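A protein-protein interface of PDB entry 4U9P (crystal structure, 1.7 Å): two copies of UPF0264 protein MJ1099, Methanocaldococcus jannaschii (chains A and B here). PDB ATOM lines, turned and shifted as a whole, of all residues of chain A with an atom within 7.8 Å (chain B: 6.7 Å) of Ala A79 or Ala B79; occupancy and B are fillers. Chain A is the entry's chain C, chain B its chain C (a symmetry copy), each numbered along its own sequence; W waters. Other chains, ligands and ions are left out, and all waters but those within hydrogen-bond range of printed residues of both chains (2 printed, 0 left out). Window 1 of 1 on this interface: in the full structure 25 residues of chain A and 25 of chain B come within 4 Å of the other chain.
The backbone carbonyl oxygen (O) of Leu B78 sits close to the backbone carbonyl oxygen (O) of Leu A78 (3.4 Å).
O of Val A66 sits at hydrogen-bond distance from OG1 of Thr B75, 2.8 Å away.
The backbone carbonyl oxygen of Val B66 is in hydrogen-bond range of the side-chain hydroxyl of Thr A75, 2.8 Å away.
The backbone carbonyl oxygen (O) of Gly A82 lies within hydrogen-bond range of the side-chain hydroxyl (OG) of Ser A86 (2.7 Å).
Thr B75 touches Ala A43 (N to CB, 3.6 Å).
Leu B78 touches Pro A46.
Leu B78 touches Ile A49.
Thr B75 touches Gly A67.
Gly A74 touches Ala B43 (CA to O, 3.4 Å).
Thr A75 touches Ala B43 (N to CB, 3.6 Å).
Thr A75 touches Ile B76 (CG2 to CD1, 3.9 Å).
CB of Ala A79 touches O of Thr B75, 3.8 Å away.
Ala A83 touches Leu B78 (N to CD2, 3.8 Å).
Ile A85 touches Val B81.
Ala A79 touches just these residues of chain B: Thr B75, Leu B78 and Ala B79.
Printed residues of chain A within 4 Å of Leu B78: Ala A43, Pro A46, Ile A49, Leu A78, Ala A79, Gly A82 and Ala A83.
Of the printed residues of chain A, Val B81 touches Pro A46 (3.9 Å), Gly A82 (3.8 Å) and Ile A85 (3.98 Å).
Of the printed residues of chain B, Ile A76 touches Thr B75.
Printed residues of chain A within 4 Å of Ala B43: Gly A74, Thr A75 and Leu A78.
Ala A114 touches none of the printed residues of chain B.
Val A69 touches none of the printed residues of chain B.
The nearest residue of chain B that does not touch Ala A79 is Gly B82 (5.3 Å).
The nearest residue of chain A that does not touch Ala B79 is Gly A82 (5.3 Å).
The nearest printed residue of chain A that does not touch Leu B78 is Thr A65 (4.1 Å).
Along chain B the printed residues that touch a printed residue of chain A span positions 43 to 83.
Among the printed residues, 28 pairs touch across the chains.
Ala A43 touches Gly B74, and with the chains exchanged Gly A74 touches Ala B43.
Ala A43 touches Leu B78, and with the chains exchanged Leu A78 touches Ala B43.
Thr A75 touches Ala B79, and with the chains exchanged Ala A79 touches Thr B75.
Val A81 touches Gly B82, and with the chains exchanged Gly A82 touches Val B81.
Water W2 lies within hydrogen-bond range of OG1 of Thr A75 (2.6 Å) and N of Ala B43 (2.8 Å).
Water W1 lies within hydrogen-bond range of OG1 of Thr B75 (2.6 Å) and N of Ala A43 (2.8 Å).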
ATOM      1  N   ALA A  43     -26.122   2.037   6.563  1.00  0.00           N
ATOM      2  CA  ALA A  43     -25.359   2.750   7.600  1.00  0.00           C
ATOM      3  C   ALA A  43     -26.224   3.183   8.776  1.00  0.00           C
ATOM      4  O   ALA A  43     -27.326   3.726   8.594  1.00  0.00           O
ATOM      5  CB  ALA A  43     -24.669   3.969   7.001  1.00  0.00           C
ATOM      6  N   PRO A  46     -24.014   8.400  13.376  1.00  0.00           N
ATOM      7  CA  PRO A  46     -22.756   8.626  14.114  1.00  0.00           C
ATOM      8  C   PRO A  46     -22.884   8.398  15.616  1.00  0.00           C
ATOM      9  O   PRO A  46     -21.987   7.830  16.221  1.00  0.00           O
ATOM     10  CB  PRO A  46     -22.382  10.091  13.794  1.00  0.00           C
ATOM     11  CG  PRO A  46     -23.549  10.677  13.126  1.00  0.00           C
ATOM     12  CD  PRO A  46     -24.333   9.546  12.501  1.00  0.00           C
ATOM     13  N   ILE A  49     -22.774   4.558  16.406  1.00  0.00           N
ATOM     14  CA  ILE A  49     -21.430   3.996  16.314  1.00  0.00           C
ATOM     15  C   ILE A  49     -20.631   4.403  17.563  1.00  0.00           C
ATOM     16  O   ILE A  49     -19.950   3.559  18.162  1.00  0.00           O
ATOM     17  CB  ILE A  49     -20.729   4.468  15.016  1.00  0.00           C
ATOM     18  CG1 ILE A  49     -21.508   3.996  13.762  1.00  0.00           C
ATOM     19  CG2 ILE A  49     -19.259   4.004  14.969  1.00  0.00           C
ATOM     20  CD1 ILE A  49     -21.095   4.717  12.441  1.00  0.00           C
ATOM     21  N   ALA A  64     -18.240  -0.724  11.359  1.00  0.00           N
ATOM     22  CA  ALA A  64     -19.426   0.058  10.980  1.00  0.00           C
ATOM     23  C   ALA A  64     -19.520   0.115   9.481  1.00  0.00           C
ATOM     24  O   ALA A  64     -18.512   0.320   8.790  1.00  0.00           O
ATOM     25  CB  ALA A  64     -19.418   1.468  11.574  1.00  0.00           C
ATOM     26  N   THR A  65     -20.731  -0.026   8.978  1.00  0.00           N
ATOM     27  CA  THR A  65     -20.969   0.050   7.544  1.00  0.00           C
ATOM     28  C   THR A  65     -21.263   1.497   7.148  1.00  0.00           C
ATOM     29  O   THR A  65     -21.838   2.259   7.950  1.00  0.00           O
ATOM     30  CB  THR A  65     -22.195  -0.820   7.192  1.00  0.00           C
ATOM     31  OG1 THR A  65     -23.299  -0.383   7.975  1.00  0.00           O
ATOM     32  CG2 THR A  65     -21.955  -2.304   7.436  1.00  0.00           C
ATOM     33  N   VAL A  66     -20.926   1.853   5.893  1.00  0.00           N
ATOM     34  CA  VAL A  66     -21.260   3.165   5.351  1.00  0.00           C
ATOM     35  C   VAL A  66     -22.435   3.080   4.367  1.00  0.00           C
ATOM     36  O   VAL A  66     -22.826   4.099   3.811  1.00  0.00           O
ATOM     37  CB  VAL A  66     -20.059   3.971   4.785  1.00  0.00           C
ATOM     38  CG1 VAL A  66     -19.066   4.300   5.893  1.00  0.00           C
ATOM     39  CG2 VAL A  66     -19.382   3.238   3.632  1.00  0.00           C
ATOM     40  N   GLY A  67     -22.970   1.879   4.161  1.00  0.00           N
ATOM     41  CA  GLY A  67     -24.142   1.657   3.322  1.00  0.00           C
ATOM     42  C   GLY A  67     -23.987   0.656   2.207  1.00  0.00           C
ATOM     43  O   GLY A  67     -22.895   0.118   2.000  1.00  0.00           O
ATOM     44  N   VAL A  69     -23.779   1.166  -0.926  1.00  0.00           N
ATOM     45  CA  VAL A  69     -23.441   2.417  -1.561  1.00  0.00           C
ATOM     46  C   VAL A  69     -23.720   2.547  -3.046  1.00  0.00           C
ATOM     47  O   VAL A  69     -23.384   1.629  -3.805  1.00  0.00           O
ATOM     48  CB  VAL A  69     -22.004   2.896  -1.200  1.00  0.00           C
ATOM     49  CG1 VAL A  69     -21.727   2.810   0.302  1.00  0.00           C
ATOM     50  CG2 VAL A  69     -20.931   2.155  -1.994  1.00  0.00           C
ATOM     51  N   LYS A  72     -20.794   6.882  -5.772  1.00  0.00           N
ATOM     52  CA  LYS A  72     -20.590   8.295  -5.429  1.00  0.00           C
ATOM     53  C   LYS A  72     -19.343   8.397  -4.571  1.00  0.00           C
ATOM     54  O   LYS A  72     -19.455   8.505  -3.338  1.00  0.00           O
ATOM     55  CB  LYS A  72     -21.799   8.882  -4.677  1.00  0.00           C
ATOM     56  CG  LYS A  72     -23.119   8.886  -5.437  1.00  0.00           C
ATOM     57  CD  LYS A  72     -24.102   9.832  -4.767  1.00  0.00           C
ATOM     58  CE  LYS A  72     -25.377  10.035  -5.550  1.00  0.00           C
ATOM     59  NZ  LYS A  72     -25.155  10.665  -6.879  1.00  0.00           N
ATOM     60  N   PRO A  73     -18.139   8.315  -5.186  1.00  0.00           N
ATOM     61  CA  PRO A  73     -16.908   8.339  -4.378  1.00  0.00           C
ATOM     62  C   PRO A  73     -16.802   9.440  -3.321  1.00  0.00           C
ATOM     63  O   PRO A  73     -16.392   9.145  -2.213  1.00  0.00           O
ATOM     64  CB  PRO A  73     -15.794   8.378  -5.434  1.00  0.00           C
ATOM     65  CG  PRO A  73     -16.385   7.715  -6.635  1.00  0.00           C
ATOM     66  CD  PRO A  73     -17.824   8.156  -6.637  1.00  0.00           C
ATOM     67  N   GLY A  74     -17.140  10.681  -3.668  1.00  0.00           N
ATOM     68  CA  GLY A  74     -17.077  11.799  -2.726  1.00  0.00           C
ATOM     69  C   GLY A  74     -17.989  11.597  -1.527  1.00  0.00           C
ATOM     70  O   GLY A  74     -17.558  11.720  -0.373  1.00  0.00           O
ATOM     71  N   THR A  75     -19.269  11.265  -1.787  1.00  0.00           N
ATOM     72  CA  THR A  75     -20.213  11.028  -0.673  1.00  0.00           C
ATOM     73  C   THR A  75     -19.724   9.931   0.257  1.00  0.00           C
ATOM     74  O   THR A  75     -19.790  10.074   1.493  1.00  0.00           O
ATOM     75  CB  THR A  75     -21.627  10.700  -1.224  1.00  0.00           C
ATOM     76  OG1 THR A  75     -22.082  11.841  -1.944  1.00  0.00           O
ATOM     77  CG2 THR A  75     -22.632  10.369  -0.091  1.00  0.00           C
ATOM     78  N   ILE A  76     -19.293   8.820  -0.337  1.00  0.00           N
ATOM     79  CA  ILE A  76     -18.868   7.659   0.425  1.00  0.00           C
ATOM     80  C   ILE A  76     -17.558   7.903   1.189  1.00  0.00           C
ATOM     81  O   ILE A  76     -17.415   7.404   2.302  1.00  0.00           O
ATOM     82  CB  ILE A  76     -18.915   6.354  -0.414  1.00  0.00           C
ATOM     83  CG1 ILE A  76     -20.326   6.162  -1.109  1.00  0.00           C
ATOM     84  CG2 ILE A  76     -18.530   5.109   0.411  1.00  0.00           C
ATOM     85  CD1 ILE A  76     -21.604   6.441  -0.175  1.00  0.00           C
ATOM     86  N   SER A  77     -16.634   8.702   0.596  1.00  0.00           N
ATOM     87  CA  SER A  77     -15.375   9.044   1.265  1.00  0.00           C
ATOM     88  C   SER A  77     -15.696   9.886   2.512  1.00  0.00           C
ATOM     89  O   SER A  77     -15.186   9.610   3.601  1.00  0.00           O
ATOM     90  CB  SER A  77     -14.446   9.792   0.310  1.00  0.00           C
ATOM     91  OG  SER A  77     -14.066   8.915  -0.745  1.00  0.00           O
ATOM     92  N   LEU A  78     -16.626  10.842   2.377  1.00  0.00           N
ATOM     93  CA  LEU A  78     -17.059  11.661   3.524  1.00  0.00           C
ATOM     94  C   LEU A  78     -17.742  10.794   4.594  1.00  0.00           C
ATOM     95  O   LEU A  78     -17.518  11.004   5.791  1.00  0.00           O
ATOM     96  CB  LEU A  78     -18.002  12.783   3.046  1.00  0.00           C
ATOM     97  CG  LEU A  78     -17.370  13.855   2.164  1.00  0.00           C
ATOM     98  CD1 LEU A  78     -18.446  14.745   1.580  1.00  0.00           C
ATOM     99  CD2 LEU A  78     -16.278  14.659   2.929  1.00  0.00           C
ATOM    100  N   ALA A  79     -18.591   9.837   4.167  1.00  0.00           N
ATOM    101  CA  ALA A  79     -19.288   8.913   5.072  1.00  0.00           C
ATOM    102  C   ALA A  79     -18.291   8.048   5.849  1.00  0.00           C
ATOM    103  O   ALA A  79     -18.445   7.884   7.064  1.00  0.00           O
ATOM    104  CB  ALA A  79     -20.265   8.030   4.291  1.00  0.00           C
ATOM    105  N   ALA A  80     -17.224   7.568   5.166  1.00  0.00           N
ATOM    106  CA  ALA A  80     -16.141   6.776   5.769  1.00  0.00           C
ATOM    107  C   ALA A  80     -15.430   7.588   6.842  1.00  0.00           C
ATOM    108  O   ALA A  80     -15.160   7.040   7.918  1.00  0.00           O
ATOM    109  CB  ALA A  80     -15.151   6.320   4.705  1.00  0.00           C
ATOM    110  N   VAL A  81     -15.223   8.920   6.595  1.00  0.00           N
ATOM    111  CA  VAL A  81     -14.664   9.849   7.590  1.00  0.00           C
ATOM    112  C   VAL A  81     -15.633   9.900   8.802  1.00  0.00           C
ATOM    113  O   VAL A  81     -15.201   9.714   9.932  1.00  0.00           O
ATOM    114  CB  VAL A  81     -14.342  11.262   7.047  1.00  0.00           C
ATOM    115  CG1 VAL A  81     -13.906  12.184   8.185  1.00  0.00           C
ATOM    116  CG2 VAL A  81     -13.259  11.207   5.971  1.00  0.00           C
ATOM    117  N   GLY A  82     -16.913  10.103   8.552  1.00  0.00           N
ATOM    118  CA  GLY A  82     -17.918  10.114   9.612  1.00  0.00           C
ATOM    119  C   GLY A  82     -17.906   8.873  10.476  1.00  0.00           C
ATOM    120  O   GLY A  82     -17.951   8.993  11.706  1.00  0.00           O
ATOM    121  N   ALA A  83     -17.777   7.680   9.854  1.00  0.00           N
ATOM    122  CA  ALA A  83     -17.767   6.394  10.580  1.00  0.00           C
ATOM    123  C   ALA A  83     -16.485   6.268  11.404  1.00  0.00           C
ATOM    124  O   ALA A  83     -16.541   5.937  12.588  1.00  0.00           O
ATOM    125  CB  ALA A  83     -17.895   5.231   9.617  1.00  0.00           C
ATOM    126  N   ALA A  84     -15.335   6.596  10.794  1.00  0.00           N
ATOM    127  CA  ALA A  84     -14.047   6.553  11.467  1.00  0.00           C
ATOM    128  C   ALA A  84     -13.991   7.485  12.689  1.00  0.00           C
ATOM    129  O   ALA A  84     -13.594   7.050  13.775  1.00  0.00           O
ATOM    130  CB  ALA A  84     -12.955   6.908  10.473  1.00  0.00           C
ATOM    131  N   ILE A  85     -14.420   8.761  12.514  1.00  0.00           N
ATOM    132  CA  ILE A  85     -14.452   9.803  13.555  1.00  0.00           C
ATOM    133  C   ILE A  85     -15.344   9.361  14.719  1.00  0.00           C
ATOM    134  O   ILE A  85     -15.006   9.605  15.881  1.00  0.00           O
ATOM    135  CB  ILE A  85     -14.923  11.161  12.907  1.00  0.00           C
ATOM    136  CG1 ILE A  85     -13.769  11.848  12.117  1.00  0.00           C
ATOM    137  CG2 ILE A  85     -15.625  12.134  13.863  1.00  0.00           C
ATOM    138  CD1 ILE A  85     -12.471  12.229  12.891  1.00  0.00           C
ATOM    139  N   SER A  86     -16.453   8.674  14.381  1.00  0.00           N
ATOM    140  CA  SER A  86     -17.443   8.153  15.334  1.00  0.00           C
ATOM    141  C   SER A  86     -16.958   6.954  16.182  1.00  0.00           C
ATOM    142  O   SER A  86     -17.626   6.592  17.152  1.00  0.00           O
ATOM    143  CB  SER A  86     -18.750   7.844  14.622  1.00  0.00           C
ATOM    144  OG  SER A  86     -19.221   9.055  14.044  1.00  0.00           O
ATOM    145  N   ILE A  91     -14.140   0.049   8.669  1.00  0.00           N
ATOM    146  CA  ILE A  91     -15.099   0.855   7.895  1.00  0.00           C
ATOM    147  C   ILE A  91     -15.487  -0.043   6.692  1.00  0.00           C
ATOM    148  O   ILE A  91     -14.632  -0.406   5.885  1.00  0.00           O
ATOM    149  CB  ILE A  91     -14.554   2.274   7.482  1.00  0.00           C
ATOM    150  CG1 ILE A  91     -14.362   3.203   8.726  1.00  0.00           C
ATOM    151  CG2 ILE A  91     -15.485   2.939   6.444  1.00  0.00           C
ATOM    152  CD1 ILE A  91     -13.115   2.936   9.515  1.00  0.00           C
ATOM    153  N   VAL A 111     -12.107   5.916  -0.488  1.00  0.00           N
ATOM    154  CA  VAL A 111     -12.490   5.584   0.888  1.00  0.00           C
ATOM    155  C   VAL A 111     -11.219   5.271   1.704  1.00  0.00           C
ATOM    156  O   VAL A 111     -11.048   5.792   2.798  1.00  0.00           O
ATOM    157  CB  VAL A 111     -13.521   4.426   0.897  1.00  0.00           C
ATOM    158  CG1 VAL A 111     -13.706   3.842   2.305  1.00  0.00           C
ATOM    159  CG2 VAL A 111     -14.864   4.890   0.317  1.00  0.00           C
ATOM    160  N   ALA A 114      -9.392   8.498   2.476  1.00  0.00           N
ATOM    161  CA  ALA A 114     -10.167   9.224   3.494  1.00  0.00           C
ATOM    162  C   ALA A 114      -9.953   8.667   4.920  1.00  0.00           C
ATOM    163  O   ALA A 114      -9.645   9.424   5.845  1.00  0.00           O
ATOM    164  CB  ALA A 114     -11.643   9.194   3.132  1.00  0.00           C
ATOM    165  N   VAL A 115     -10.036   7.337   5.065  1.00  0.00           N
ATOM    166  CA  VAL A 115      -9.845   6.632   6.335  1.00  0.00           C
ATOM    167  C   VAL A 115      -8.393   6.738   6.830  1.00  0.00           C
ATOM    168  O   VAL A 115      -8.186   7.078   7.995  1.00  0.00           O
ATOM    169  CB  VAL A 115     -10.357   5.175   6.258  1.00  0.00           C
ATOM    170  CG1 VAL A 115     -10.087   4.410   7.573  1.00  0.00           C
ATOM    171  CG2 VAL A 115     -11.855   5.147   5.928  1.00  0.00           C
ATOM    172  N   ALA B  43     -20.759  15.508  -4.098  1.00  0.00           N
ATOM    173  CA  ALA B  43     -19.779  15.766  -3.032  1.00  0.00           C
ATOM    174  C   ALA B  43     -18.339  15.654  -3.513  1.00  0.00           C
ATOM    175  O   ALA B  43     -17.973  14.700  -4.220  1.00  0.00           O
ATOM    176  CB  ALA B  43     -20.002  14.807  -1.868  1.00  0.00           C
ATOM    177  N   THR B  65     -20.977  20.453  -0.270  1.00  0.00           N
ATOM    178  CA  THR B  65     -22.131  19.601  -0.517  1.00  0.00           C
ATOM    179  C   THR B  65     -21.813  18.167  -0.091  1.00  0.00           C
ATOM    180  O   THR B  65     -20.647  17.735  -0.180  1.00  0.00           O
ATOM    181  CB  THR B  65     -22.449  19.611  -2.028  1.00  0.00           C
ATOM    182  OG1 THR B  65     -21.284  19.208  -2.737  1.00  0.00           O
ATOM    183  CG2 THR B  65     -22.901  20.978  -2.526  1.00  0.00           C
ATOM    184  N   VAL B  66     -22.858  17.416   0.310  1.00  0.00           N
ATOM    185  CA  VAL B  66     -22.709  16.001   0.627  1.00  0.00           C
ATOM    186  C   VAL B  66     -23.277  15.116  -0.491  1.00  0.00           C
ATOM    187  O   VAL B  66     -23.243  13.898  -0.366  1.00  0.00           O
ATOM    188  CB  VAL B  66     -23.212  15.585   2.037  1.00  0.00           C
ATOM    189  CG1 VAL B  66     -22.388  16.268   3.122  1.00  0.00           C
ATOM    190  CG2 VAL B  66     -24.700  15.866   2.210  1.00  0.00           C
ATOM    191  N   GLY B  74     -28.693   7.448   7.397  1.00  0.00           N
ATOM    192  CA  GLY B  74     -27.439   7.063   8.045  1.00  0.00           C
ATOM    193  C   GLY B  74     -26.221   7.436   7.215  1.00  0.00           C
ATOM    194  O   GLY B  74     -25.285   8.074   7.712  1.00  0.00           O
ATOM    195  N   THR B  75     -26.227   7.051   5.923  1.00  0.00           N
ATOM    196  CA  THR B  75     -25.089   7.397   5.043  1.00  0.00           C
ATOM    197  C   THR B  75     -24.855   8.896   4.986  1.00  0.00           C
ATOM    198  O   THR B  75     -23.701   9.359   5.064  1.00  0.00           O
ATOM    199  CB  THR B  75     -25.310   6.814   3.621  1.00  0.00           C
ATOM    200  OG1 THR B  75     -25.353   5.395   3.741  1.00  0.00           O
ATOM    201  CG2 THR B  75     -24.176   7.217   2.643  1.00  0.00           C
ATOM    202  N   ILE B  76     -25.940   9.643   4.791  1.00  0.00           N
ATOM    203  CA  ILE B  76     -25.861  11.086   4.638  1.00  0.00           C
ATOM    204  C   ILE B  76     -25.459  11.794   5.939  1.00  0.00           C
ATOM    205  O   ILE B  76     -24.728  12.780   5.881  1.00  0.00           O
ATOM    206  CB  ILE B  76     -27.105  11.671   3.918  1.00  0.00           C
ATOM    207  CG1 ILE B  76     -27.397  10.913   2.557  1.00  0.00           C
ATOM    208  CG2 ILE B  76     -26.993  13.192   3.693  1.00  0.00           C
ATOM    209  CD1 ILE B  76     -26.116  10.636   1.627  1.00  0.00           C
ATOM    210  N   SER B  77     -25.911  11.259   7.102  1.00  0.00           N
ATOM    211  CA  SER B  77     -25.538  11.825   8.402  1.00  0.00           C
ATOM    212  C   SER B  77     -24.022  11.649   8.598  1.00  0.00           C
ATOM    213  O   SER B  77     -23.325  12.598   8.966  1.00  0.00           O
ATOM    214  CB  SER B  77     -26.328  11.155   9.526  1.00  0.00           C
ATOM    215  OG  SER B  77     -27.707  11.475   9.375  1.00  0.00           O
ATOM    216  N   LEU B  78     -23.497  10.467   8.243  1.00  0.00           N
ATOM    217  CA  LEU B  78     -22.046  10.215   8.324  1.00  0.00           C
ATOM    218  C   LEU B  78     -21.273  11.132   7.364  1.00  0.00           C
ATOM    219  O   LEU B  78     -20.207  11.641   7.725  1.00  0.00           O
ATOM    220  CB  LEU B  78     -21.751   8.733   8.022  1.00  0.00           C
ATOM    221  CG  LEU B  78     -22.263   7.727   9.047  1.00  0.00           C
ATOM    222  CD1 LEU B  78     -22.117   6.319   8.510  1.00  0.00           C
ATOM    223  CD2 LEU B  78     -21.575   7.915  10.431  1.00  0.00           C
ATOM    224  N   ALA B  79     -21.795  11.325   6.136  1.00  0.00           N
ATOM    225  CA  ALA B  79     -21.185  12.202   5.126  1.00  0.00           C
ATOM    226  C   ALA B  79     -21.132  13.651   5.616  1.00  0.00           C
ATOM    227  O   ALA B  79     -20.095  14.306   5.467  1.00  0.00           O
ATOM    228  CB  ALA B  79     -21.951  12.114   3.803  1.00  0.00           C
ATOM    229  N   ALA B  80     -22.217  14.122   6.278  1.00  0.00           N
ATOM    230  CA  ALA B  80     -22.310  15.465   6.870  1.00  0.00           C
ATOM    231  C   ALA B  80     -21.244  15.643   7.942  1.00  0.00           C
ATOM    232  O   ALA B  80     -20.601  16.699   7.968  1.00  0.00           O
ATOM    233  CB  ALA B  80     -23.696  15.700   7.455  1.00  0.00           C
ATOM    234  N   VAL B  81     -20.980  14.573   8.756  1.00  0.00           N
ATOM    235  CA  VAL B  81     -19.893  14.560   9.748  1.00  0.00           C
ATOM    236  C   VAL B  81     -18.547  14.720   8.992  1.00  0.00           C
ATOM    237  O   VAL B  81     -17.756  15.587   9.338  1.00  0.00           O
ATOM    238  CB  VAL B  81     -19.887  13.331  10.687  1.00  0.00           C
ATOM    239  CG1 VAL B  81     -18.644  13.344  11.575  1.00  0.00           C
ATOM    240  CG2 VAL B  81     -21.148  13.286  11.548  1.00  0.00           C
ATOM    241  N   GLY B  82     -18.328  13.926   7.960  1.00  0.00           N
ATOM    242  CA  GLY B  82     -17.120  14.028   7.145  1.00  0.00           C
ATOM    243  C   GLY B  82     -16.870  15.415   6.598  1.00  0.00           C
ATOM    244  O   GLY B  82     -15.736  15.902   6.683  1.00  0.00           O
ATOM    245  N   ALA B  83     -17.929  16.091   6.098  1.00  0.00           N
ATOM    246  CA  ALA B  83     -17.816  17.444   5.520  1.00  0.00           C
ATOM    247  C   ALA B  83     -17.503  18.458   6.621  1.00  0.00           C
ATOM    248  O   ALA B  83     -16.588  19.269   6.474  1.00  0.00           O
ATOM    249  CB  ALA B  83     -19.088  17.827   4.792  1.00  0.00           C
ATOM    250  N   ALA B  84     -18.222  18.371   7.751  1.00  0.00           N
ATOM    251  CA  ALA B  84     -18.010  19.250   8.890  1.00  0.00           C
ATOM    252  C   ALA B  84     -16.583  19.143   9.456  1.00  0.00           C
ATOM    253  O   ALA B  84     -15.921  20.168   9.649  1.00  0.00           O
ATOM    254  CB  ALA B  84     -19.036  18.932   9.963  1.00  0.00           C
ATOM    255  N   ILE B  91     -23.043  22.898   5.500  1.00  0.00           N
ATOM    256  CA  ILE B  91     -23.128  21.511   5.014  1.00  0.00           C
ATOM    257  C   ILE B  91     -24.432  21.466   4.176  1.00  0.00           C
ATOM    258  O   ILE B  91     -25.519  21.700   4.702  1.00  0.00           O
ATOM    259  CB  ILE B  91     -23.068  20.429   6.157  1.00  0.00           C
ATOM    260  CG1 ILE B  91     -21.662  20.390   6.842  1.00  0.00           C
ATOM    261  CG2 ILE B  91     -23.448  19.033   5.614  1.00  0.00           C
ATOM    262  CD1 ILE B  91     -21.427  21.483   7.842  1.00  0.00           C
HETATM  263  O   HOH W   1     -27.112   3.545   4.378  1.00  0.00           O
HETATM  264  O   HOH W   2     -21.783  12.878  -4.345  1.00  0.00           O
